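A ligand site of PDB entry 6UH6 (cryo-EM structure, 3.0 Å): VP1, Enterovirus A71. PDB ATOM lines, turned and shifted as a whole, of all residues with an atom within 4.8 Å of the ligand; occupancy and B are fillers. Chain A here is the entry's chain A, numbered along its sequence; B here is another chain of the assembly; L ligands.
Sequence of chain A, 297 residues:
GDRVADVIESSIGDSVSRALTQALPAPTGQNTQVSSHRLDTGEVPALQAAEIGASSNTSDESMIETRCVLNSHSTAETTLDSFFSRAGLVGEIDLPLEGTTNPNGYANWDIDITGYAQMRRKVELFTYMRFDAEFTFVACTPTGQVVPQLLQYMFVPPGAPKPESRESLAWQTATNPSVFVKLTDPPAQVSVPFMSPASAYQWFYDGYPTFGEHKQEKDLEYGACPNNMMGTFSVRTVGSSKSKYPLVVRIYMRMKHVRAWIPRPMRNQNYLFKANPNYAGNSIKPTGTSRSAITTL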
ATOM      1  N   ILE A 111      28.914   9.378 -26.945  1.00  0.00           N
ATOM      2  CA  ILE A 111      28.080   8.205 -26.749  1.00  0.00           C
ATOM      3  C   ILE A 111      28.944   6.966 -26.806  1.00  0.00           C
ATOM      4  O   ILE A 111      29.444   6.583 -27.873  1.00  0.00           O
ATOM      5  CB  ILE A 111      26.951   8.141 -27.782  1.00  0.00           C
ATOM      6  CG1 ILE A 111      26.137   9.430 -27.773  1.00  0.00           C
ATOM      7  CG2 ILE A 111      26.064   6.916 -27.523  1.00  0.00           C
ATOM      8  CD1 ILE A 111      25.126   9.517 -28.829  1.00  0.00           C
ATOM      9  N   ASP A 112      29.118   6.328 -25.666  1.00  0.00           N
ATOM     10  CA  ASP A 112      29.493   4.927 -25.616  1.00  0.00           C
ATOM     11  C   ASP A 112      28.746   4.318 -24.446  1.00  0.00           C
ATOM     12  O   ASP A 112      28.750   4.861 -23.349  1.00  0.00           O
ATOM     13  CB  ASP A 112      31.014   4.736 -25.506  1.00  0.00           C
ATOM     14  CG  ASP A 112      31.572   5.215 -24.196  1.00  0.00           C
ATOM     15  OD1 ASP A 112      31.035   6.187 -23.627  1.00  0.00           O
ATOM     16  OD2 ASP A 112      32.559   4.619 -23.738  1.00  0.00           O
ATOM     17  N   ILE A 113      28.097   3.192 -24.706  1.00  0.00           N
ATOM     18  CA  ILE A 113      27.304   2.506 -23.702  1.00  0.00           C
ATOM     19  C   ILE A 113      28.140   1.475 -22.967  1.00  0.00           C
ATOM     20  O   ILE A 113      27.598   0.535 -22.385  1.00  0.00           O
ATOM     21  CB  ILE A 113      26.025   1.915 -24.323  1.00  0.00           C
ATOM     22  CG1 ILE A 113      26.287   0.648 -25.154  1.00  0.00           C
ATOM     23  CG2 ILE A 113      25.383   2.969 -25.200  1.00  0.00           C
ATOM     24  CD1 ILE A 113      25.038  -0.064 -25.652  1.00  0.00           C
ATOM     25  N   THR A 114      29.458   1.635 -22.975  1.00  0.00           N
ATOM     26  CA  THR A 114      30.425   0.697 -22.433  1.00  0.00           C
ATOM     27  C   THR A 114      31.165   1.299 -21.243  1.00  0.00           C
ATOM     28  O   THR A 114      32.372   1.127 -21.089  1.00  0.00           O
ATOM     29  CB  THR A 114      31.419   0.284 -23.503  1.00  0.00           C
ATOM     30  OG1 THR A 114      32.209   1.400 -23.879  1.00  0.00           O
ATOM     31  CG2 THR A 114      30.690  -0.227 -24.725  1.00  0.00           C
ATOM     32  N   PHE A 131      19.594  -2.299 -33.760  1.00  0.00           N
ATOM     33  CA  PHE A 131      18.427  -1.992 -32.962  1.00  0.00           C
ATOM     34  C   PHE A 131      18.093  -0.511 -33.005  1.00  0.00           C
ATOM     35  O   PHE A 131      18.975   0.341 -33.142  1.00  0.00           O
ATOM     36  CB  PHE A 131      18.617  -2.435 -31.509  1.00  0.00           C
ATOM     37  CG  PHE A 131      19.842  -1.885 -30.861  1.00  0.00           C
ATOM     38  CD1 PHE A 131      19.829  -0.664 -30.250  1.00  0.00           C
ATOM     39  CD2 PHE A 131      20.986  -2.625 -30.817  1.00  0.00           C
ATOM     40  CE1 PHE A 131      20.940  -0.183 -29.656  1.00  0.00           C
ATOM     41  CE2 PHE A 131      22.103  -2.134 -30.215  1.00  0.00           C
ATOM     42  CZ  PHE A 131      22.072  -0.913 -29.628  1.00  0.00           C
ATOM     43  N   PHE A 135      16.039   6.358 -25.293  1.00  0.00           N
ATOM     44  CA  PHE A 135      16.815   6.992 -24.240  1.00  0.00           C
ATOM     45  C   PHE A 135      15.885   7.737 -23.299  1.00  0.00           C
ATOM     46  O   PHE A 135      14.787   8.143 -23.691  1.00  0.00           O
ATOM     47  CB  PHE A 135      17.840   7.932 -24.840  1.00  0.00           C
ATOM     48  CG  PHE A 135      18.985   7.232 -25.455  1.00  0.00           C
ATOM     49  CD1 PHE A 135      18.907   6.721 -26.720  1.00  0.00           C
ATOM     50  CD2 PHE A 135      20.141   7.051 -24.742  1.00  0.00           C
ATOM     51  CE1 PHE A 135      19.949   6.070 -27.270  1.00  0.00           C
ATOM     52  CE2 PHE A 135      21.191   6.400 -25.299  1.00  0.00           C
ATOM     53  CZ  PHE A 135      21.097   5.919 -26.552  1.00  0.00           C
ATOM     54  N   PHE A 137      16.179  10.412 -19.741  1.00  0.00           N
ATOM     55  CA  PHE A 137      17.089  11.302 -19.043  1.00  0.00           C
ATOM     56  C   PHE A 137      16.482  11.650 -17.700  1.00  0.00           C
ATOM     57  O   PHE A 137      15.443  12.309 -17.635  1.00  0.00           O
ATOM     58  CB  PHE A 137      17.378  12.545 -19.880  1.00  0.00           C
ATOM     59  CG  PHE A 137      17.752  12.227 -21.287  1.00  0.00           C
ATOM     60  CD1 PHE A 137      19.056  12.023 -21.626  1.00  0.00           C
ATOM     61  CD2 PHE A 137      16.793  12.092 -22.260  1.00  0.00           C
ATOM     62  CE1 PHE A 137      19.396  11.713 -22.910  1.00  0.00           C
ATOM     63  CE2 PHE A 137      17.125  11.772 -23.538  1.00  0.00           C
ATOM     64  CZ  PHE A 137      18.432  11.577 -23.855  1.00  0.00           C
ATOM     65  N   TYR A 153      18.789  19.411 -24.020  1.00  0.00           N
ATOM     66  CA  TYR A 153      19.458  18.166 -24.380  1.00  0.00           C
ATOM     67  C   TYR A 153      19.640  18.150 -25.891  1.00  0.00           C
ATOM     68  O   TYR A 153      18.708  17.791 -26.627  1.00  0.00           O
ATOM     69  CB  TYR A 153      18.651  16.949 -23.944  1.00  0.00           C
ATOM     70  CG  TYR A 153      18.430  16.746 -22.472  1.00  0.00           C
ATOM     71  CD1 TYR A 153      19.404  17.052 -21.544  1.00  0.00           C
ATOM     72  CD2 TYR A 153      17.257  16.219 -22.017  1.00  0.00           C
ATOM     73  CE1 TYR A 153      19.191  16.851 -20.213  1.00  0.00           C
ATOM     74  CE2 TYR A 153      17.045  16.008 -20.686  1.00  0.00           C
ATOM     75  CZ  TYR A 153      18.003  16.324 -19.796  1.00  0.00           C
ATOM     76  OH  TYR A 153      17.762  16.103 -18.470  1.00  0.00           O
ATOM     77  N   PHE A 155      21.493  16.714 -29.341  1.00  0.00           N
ATOM     78  CA  PHE A 155      22.222  15.645 -30.004  1.00  0.00           C
ATOM     79  C   PHE A 155      23.073  16.262 -31.101  1.00  0.00           C
ATOM     80  O   PHE A 155      22.555  16.916 -32.001  1.00  0.00           O
ATOM     81  CB  PHE A 155      21.265  14.623 -30.583  1.00  0.00           C
ATOM     82  CG  PHE A 155      21.916  13.546 -31.386  1.00  0.00           C
ATOM     83  CD1 PHE A 155      23.106  12.970 -30.990  1.00  0.00           C
ATOM     84  CD2 PHE A 155      21.327  13.104 -32.536  1.00  0.00           C
ATOM     85  CE1 PHE A 155      23.678  11.992 -31.747  1.00  0.00           C
ATOM     86  CE2 PHE A 155      21.899  12.136 -33.293  1.00  0.00           C
ATOM     87  CZ  PHE A 155      23.067  11.570 -32.893  1.00  0.00           C
ATOM     88  N   PRO A 177      18.672  17.910 -33.579  1.00  0.00           N
ATOM     89  CA  PRO A 177      17.544  17.705 -32.668  1.00  0.00           C
ATOM     90  C   PRO A 177      17.901  18.023 -31.227  1.00  0.00           C
ATOM     91  O   PRO A 177      18.978  17.656 -30.745  1.00  0.00           O
ATOM     92  CB  PRO A 177      17.196  16.228 -32.845  1.00  0.00           C
ATOM     93  CG  PRO A 177      18.281  15.619 -33.539  1.00  0.00           C
ATOM     94  CD  PRO A 177      19.251  16.627 -34.010  1.00  0.00           C
ATOM     95  N   VAL A 179      16.011  18.848 -27.076  1.00  0.00           N
ATOM     96  CA  VAL A 179      14.903  18.663 -26.155  1.00  0.00           C
ATOM     97  C   VAL A 179      15.066  19.655 -25.020  1.00  0.00           C
ATOM     98  O   VAL A 179      16.156  19.797 -24.477  1.00  0.00           O
ATOM     99  CB  VAL A 179      14.825  17.224 -25.625  1.00  0.00           C
ATOM    100  CG1 VAL A 179      14.019  17.145 -24.391  1.00  0.00           C
ATOM    101  CG2 VAL A 179      14.212  16.320 -26.628  1.00  0.00           C
ATOM    102  N   VAL A 190      12.881   9.872 -25.553  1.00  0.00           N
ATOM    103  CA  VAL A 190      12.841   9.915 -27.011  1.00  0.00           C
ATOM    104  C   VAL A 190      13.188   8.543 -27.559  1.00  0.00           C
ATOM    105  O   VAL A 190      13.967   7.784 -26.964  1.00  0.00           O
ATOM    106  CB  VAL A 190      13.778  10.984 -27.594  1.00  0.00           C
ATOM    107  CG1 VAL A 190      13.253  12.340 -27.325  1.00  0.00           C
ATOM    108  CG2 VAL A 190      15.155  10.886 -27.018  1.00  0.00           C
ATOM    109  N   VAL A 192      14.741   6.436 -30.937  1.00  0.00           N
ATOM    110  CA  VAL A 192      15.909   6.680 -31.777  1.00  0.00           C
ATOM    111  C   VAL A 192      15.929   5.596 -32.849  1.00  0.00           C
ATOM    112  O   VAL A 192      15.520   4.472 -32.580  1.00  0.00           O
ATOM    113  CB  VAL A 192      17.216   6.667 -30.974  1.00  0.00           C
ATOM    114  CG1 VAL A 192      18.354   6.932 -31.854  1.00  0.00           C
ATOM    115  CG2 VAL A 192      17.176   7.701 -29.912  1.00  0.00           C
ATOM    116  N   MET A 195      21.182   4.178 -36.734  1.00  0.00           N
ATOM    117  CA  MET A 195      21.763   5.368 -37.327  1.00  0.00           C
ATOM    118  C   MET A 195      23.189   5.167 -37.855  1.00  0.00           C
ATOM    119  O   MET A 195      23.905   6.140 -38.079  1.00  0.00           O
ATOM    120  CB  MET A 195      21.765   6.502 -36.307  1.00  0.00           C
ATOM    121  CG  MET A 195      20.406   7.027 -35.972  1.00  0.00           C
ATOM    122  SD  MET A 195      20.425   8.707 -35.377  1.00  0.00           S
ATOM    123  CE  MET A 195      21.564   8.477 -34.046  1.00  0.00           C
ATOM    124  N   TYR A 201      25.698  -2.227 -35.716  1.00  0.00           N
ATOM    125  CA  TYR A 201      26.768  -1.891 -34.809  1.00  0.00           C
ATOM    126  C   TYR A 201      27.609  -3.125 -34.526  1.00  0.00           C
ATOM    127  O   TYR A 201      27.176  -4.252 -34.747  1.00  0.00           O
ATOM    128  CB  TYR A 201      26.223  -1.342 -33.496  1.00  0.00           C
ATOM    129  CG  TYR A 201      25.317  -0.160 -33.631  1.00  0.00           C
ATOM    130  CD1 TYR A 201      25.820   1.095 -33.906  1.00  0.00           C
ATOM    131  CD2 TYR A 201      23.963  -0.302 -33.485  1.00  0.00           C
ATOM    132  CE1 TYR A 201      24.991   2.167 -34.039  1.00  0.00           C
ATOM    133  CE2 TYR A 201      23.128   0.770 -33.625  1.00  0.00           C
ATOM    134  CZ  TYR A 201      23.645   1.994 -33.898  1.00  0.00           C
ATOM    135  OH  TYR A 201      22.792   3.056 -34.013  1.00  0.00           O
ATOM    136  N   TRP A 203      30.542  -4.272 -31.473  1.00  0.00           N
ATOM    137  CA  TRP A 203      31.250  -3.881 -30.263  1.00  0.00           C
ATOM    138  C   TRP A 203      32.704  -4.310 -30.282  1.00  0.00           C
ATOM    139  O   TRP A 203      33.485  -3.863 -29.446  1.00  0.00           O
ATOM    140  CB  TRP A 203      30.567  -4.480 -29.040  1.00  0.00           C
ATOM    141  CG  TRP A 203      29.088  -4.499 -29.146  1.00  0.00           C
ATOM    142  CD1 TRP A 203      28.327  -5.575 -29.424  1.00  0.00           C
ATOM    143  CD2 TRP A 203      28.204  -3.401 -29.015  1.00  0.00           C
ATOM    144  NE1 TRP A 203      27.019  -5.225 -29.477  1.00  0.00           N
ATOM    145  CE2 TRP A 203      26.904  -3.888 -29.223  1.00  0.00           C
ATOM    146  CE3 TRP A 203      28.373  -2.045 -28.746  1.00  0.00           C
ATOM    147  CZ2 TRP A 203      25.787  -3.080 -29.161  1.00  0.00           C
ATOM    148  CZ3 TRP A 203      27.262  -1.247 -28.676  1.00  0.00           C
ATOM    149  CH2 TRP A 203      25.984  -1.764 -28.888  1.00  0.00           C
ATOM    150  N   ASN A 228      30.230   3.149 -35.333  1.00  0.00           N
ATOM    151  CA  ASN A 228      29.559   3.149 -34.049  1.00  0.00           C
ATOM    152  C   ASN A 228      29.546   4.508 -33.385  1.00  0.00           C
ATOM    153  O   ASN A 228      28.771   4.713 -32.443  1.00  0.00           O
ATOM    154  CB  ASN A 228      30.251   2.154 -33.120  1.00  0.00           C
ATOM    155  CG  ASN A 228      29.911   0.739 -33.438  1.00  0.00           C
ATOM    156  OD1 ASN A 228      29.272   0.444 -34.450  1.00  0.00           O
ATOM    157  ND2 ASN A 228      30.344  -0.154 -32.591  1.00  0.00           N
ATOM    158  N   MET A 229      30.391   5.426 -33.842  1.00  0.00           N
ATOM    159  CA  MET A 229      30.464   6.757 -33.280  1.00  0.00           C
ATOM    160  C   MET A 229      29.294   7.555 -33.799  1.00  0.00           C
ATOM    161  O   MET A 229      29.377   8.212 -34.842  1.00  0.00           O
ATOM    162  CB  MET A 229      31.788   7.403 -33.645  1.00  0.00           C
ATOM    163  CG  MET A 229      32.960   6.685 -33.089  1.00  0.00           C
ATOM    164  SD  MET A 229      34.536   7.461 -33.414  1.00  0.00           S
ATOM    165  CE  MET A 229      35.589   6.171 -32.792  1.00  0.00           C
ATOM    166  N   MET A 230      28.188   7.514 -33.075  1.00  0.00           N
ATOM    167  CA  MET A 230      26.974   8.209 -33.452  1.00  0.00           C
ATOM    168  C   MET A 230      26.979   9.652 -32.999  1.00  0.00           C
ATOM    169  O   MET A 230      26.016  10.377 -33.287  1.00  0.00           O
ATOM    170  CB  MET A 230      25.754   7.490 -32.879  1.00  0.00           C
ATOM    171  CG  MET A 230      25.433   6.149 -33.507  1.00  0.00           C
ATOM    172  SD  MET A 230      25.102   6.207 -35.261  1.00  0.00           S
ATOM    173  CE  MET A 230      26.715   5.757 -35.892  1.00  0.00           C
ATOM    174  N   PHE A 233      26.277  13.771 -27.140  1.00  0.00           N
ATOM    175  CA  PHE A 233      25.099  14.270 -26.455  1.00  0.00           C
ATOM    176  C   PHE A 233      25.561  15.396 -25.536  1.00  0.00           C
ATOM    177  O   PHE A 233      26.373  15.172 -24.634  1.00  0.00           O
ATOM    178  CB  PHE A 233      24.419  13.158 -25.676  1.00  0.00           C
ATOM    179  CG  PHE A 233      23.354  13.623 -24.752  1.00  0.00           C
ATOM    180  CD1 PHE A 233      22.079  13.810 -25.203  1.00  0.00           C
ATOM    181  CD2 PHE A 233      23.638  13.872 -23.431  1.00  0.00           C
ATOM    182  CE1 PHE A 233      21.108  14.236 -24.373  1.00  0.00           C
ATOM    183  CE2 PHE A 233      22.664  14.309 -22.587  1.00  0.00           C
ATOM    184  CZ  PHE A 233      21.397  14.496 -23.044  1.00  0.00           C
ATOM    185  N   ALA A 275      35.580   0.511 -24.503  1.00  0.00           N
ATOM    186  CA  ALA A 275      35.901   0.062 -25.849  1.00  0.00           C
ATOM    187  C   ALA A 275      37.270  -0.607 -25.920  1.00  0.00           C
ATOM    188  O   ALA A 275      38.038  -0.402 -26.865  1.00  0.00           O
ATOM    189  CB  ALA A 275      35.834   1.217 -26.836  1.00  0.00           C
ATOM    190  N   ILE B  24      13.104  11.564 -32.684  1.00  0.00           N
ATOM    191  CA  ILE B  24      13.882  12.777 -32.888  1.00  0.00           C
ATOM    192  C   ILE B  24      14.053  13.110 -34.359  1.00  0.00           C
ATOM    193  O   ILE B  24      14.160  14.286 -34.718  1.00  0.00           O
ATOM    194  CB  ILE B  24      15.265  12.667 -32.204  1.00  0.00           C
ATOM    195  CG1 ILE B  24      15.936  11.341 -32.494  1.00  0.00           C
ATOM    196  CG2 ILE B  24      15.124  12.834 -30.735  1.00  0.00           C
ATOM    197  CD1 ILE B  24      17.429  11.349 -32.335  1.00  0.00           C
HETATM  198  C1  LIG L   1      31.201   1.530 -29.635  1.00  0.00           C
HETATM  199  O1  LIG L   1      31.793   0.744 -28.618  1.00  0.00           O
HETATM  200  C2  LIG L   1      30.136   2.471 -29.076  1.00  0.00           C
HETATM  201  N1  LIG L   1      30.102   3.743 -29.813  1.00  0.00           N
HETATM  202  C3  LIG L   1      28.760   1.790 -29.020  1.00  0.00           C
HETATM  203  O2  LIG L   1      28.215   1.879 -27.714  1.00  0.00           O
HETATM  204  C4  LIG L   1      27.812   2.405 -30.015  1.00  0.00           C
HETATM  205  C5  LIG L   1      26.817   3.180 -29.720  1.00  0.00           C
HETATM  206  C6  LIG L   1      25.524   2.740 -29.089  1.00  0.00           C
HETATM  207  C7  LIG L   1      24.356   2.874 -30.004  1.00  0.00           C
HETATM  208  C8  LIG L   1      24.018   4.300 -30.391  1.00  0.00           C
HETATM  209  C9  LIG L   1      22.605   4.715 -30.081  1.00  0.00           C
HETATM  210  C10 LIG L   1      22.203   6.054 -30.658  1.00  0.00           C
HETATM  211  C11 LIG L   1      22.589   7.231 -29.807  1.00  0.00           C
HETATM  212  C12 LIG L   1      21.875   8.516 -30.169  1.00  0.00           C
HETATM  213  C13 LIG L   1      21.634   9.448 -29.011  1.00  0.00           C
HETATM  214  C14 LIG L   1      20.312  10.169 -29.061  1.00  0.00           C
HETATM  215  C15 LIG L   1      20.173  11.283 -28.049  1.00  0.00           C
HETATM  216  C16 LIG L   1      18.971  12.166 -28.270  1.00  0.00           C
HETATM  217  C17 LIG L   1      19.007  13.465 -27.507  1.00  0.00           C
HETATM  218  C18 LIG L   1      17.856  14.389 -27.828  1.00  0.00           C
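The backbone carbonyl oxygen (O) of Asn 228 is in hydrogen-bond range of a nitrogen (N1) of the ligand, at 3.1 Å.
The backbone NH (N) of Ile 113 sits at hydrogen-bond distance from an oxygen (O2) of the ligand.
The backbone NH of Tyr 153 lies within hydrogen-bond range of the backbone carbonyl oxygen of Val 179 (2.7 Å).
The backbone NH (N) of Phe 135 is in hydrogen-bond range of the backbone carbonyl oxygen (O) of Val 190 (3.0 Å).
The backbone NH (N) of Met 195 is in hydrogen-bond range of the side-chain hydroxyl (OH) of Tyr 201 (3.4 Å).
The side-chain hydroxyl of Thr 114 lies within hydrogen-bond range of the side-chain carboxylate of Asp 112, at 3.2 Å.
The backbone carbonyl oxygen (O) of Pro 177 lies within hydrogen-bond range of the backbone NH (N) of Phe 155, 3.0 Å away.
CD1 of Ile 111 touches C13 of the ligand (3.5 Å).
Asp 112 touches the ligand (CA to O2, 3.9 Å).
CZ of Phe 135 touches C11 of the ligand, 3.8 Å away.
O of Tyr 153 touches C18 of the ligand (3.7 Å).
CB of Phe 155 touches C17 of the ligand, at 3.99 Å.
Met 195 touches the ligand.
CZ3 of Trp 203 touches C3 of the ligand, 3.4 Å away.
Met 230 touches the ligand (CG to C8, 3.9 Å).
Phe 233 touches the ligand (CE1 to C17, 3.9 Å).
Hydrophobic or aromatic side chains that line the ligand: Ile 111, Ile 113, Phe 135, Phe 155, Met 195, Trp 203, Met 230 and Phe 233.
Within 4 Å of the ligand: Ile 111, Asp 112, Ile 113, Phe 135, Tyr 153, Phe 155, Met 195, Trp 203, Asn 228, Met 230 and Phe 233.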
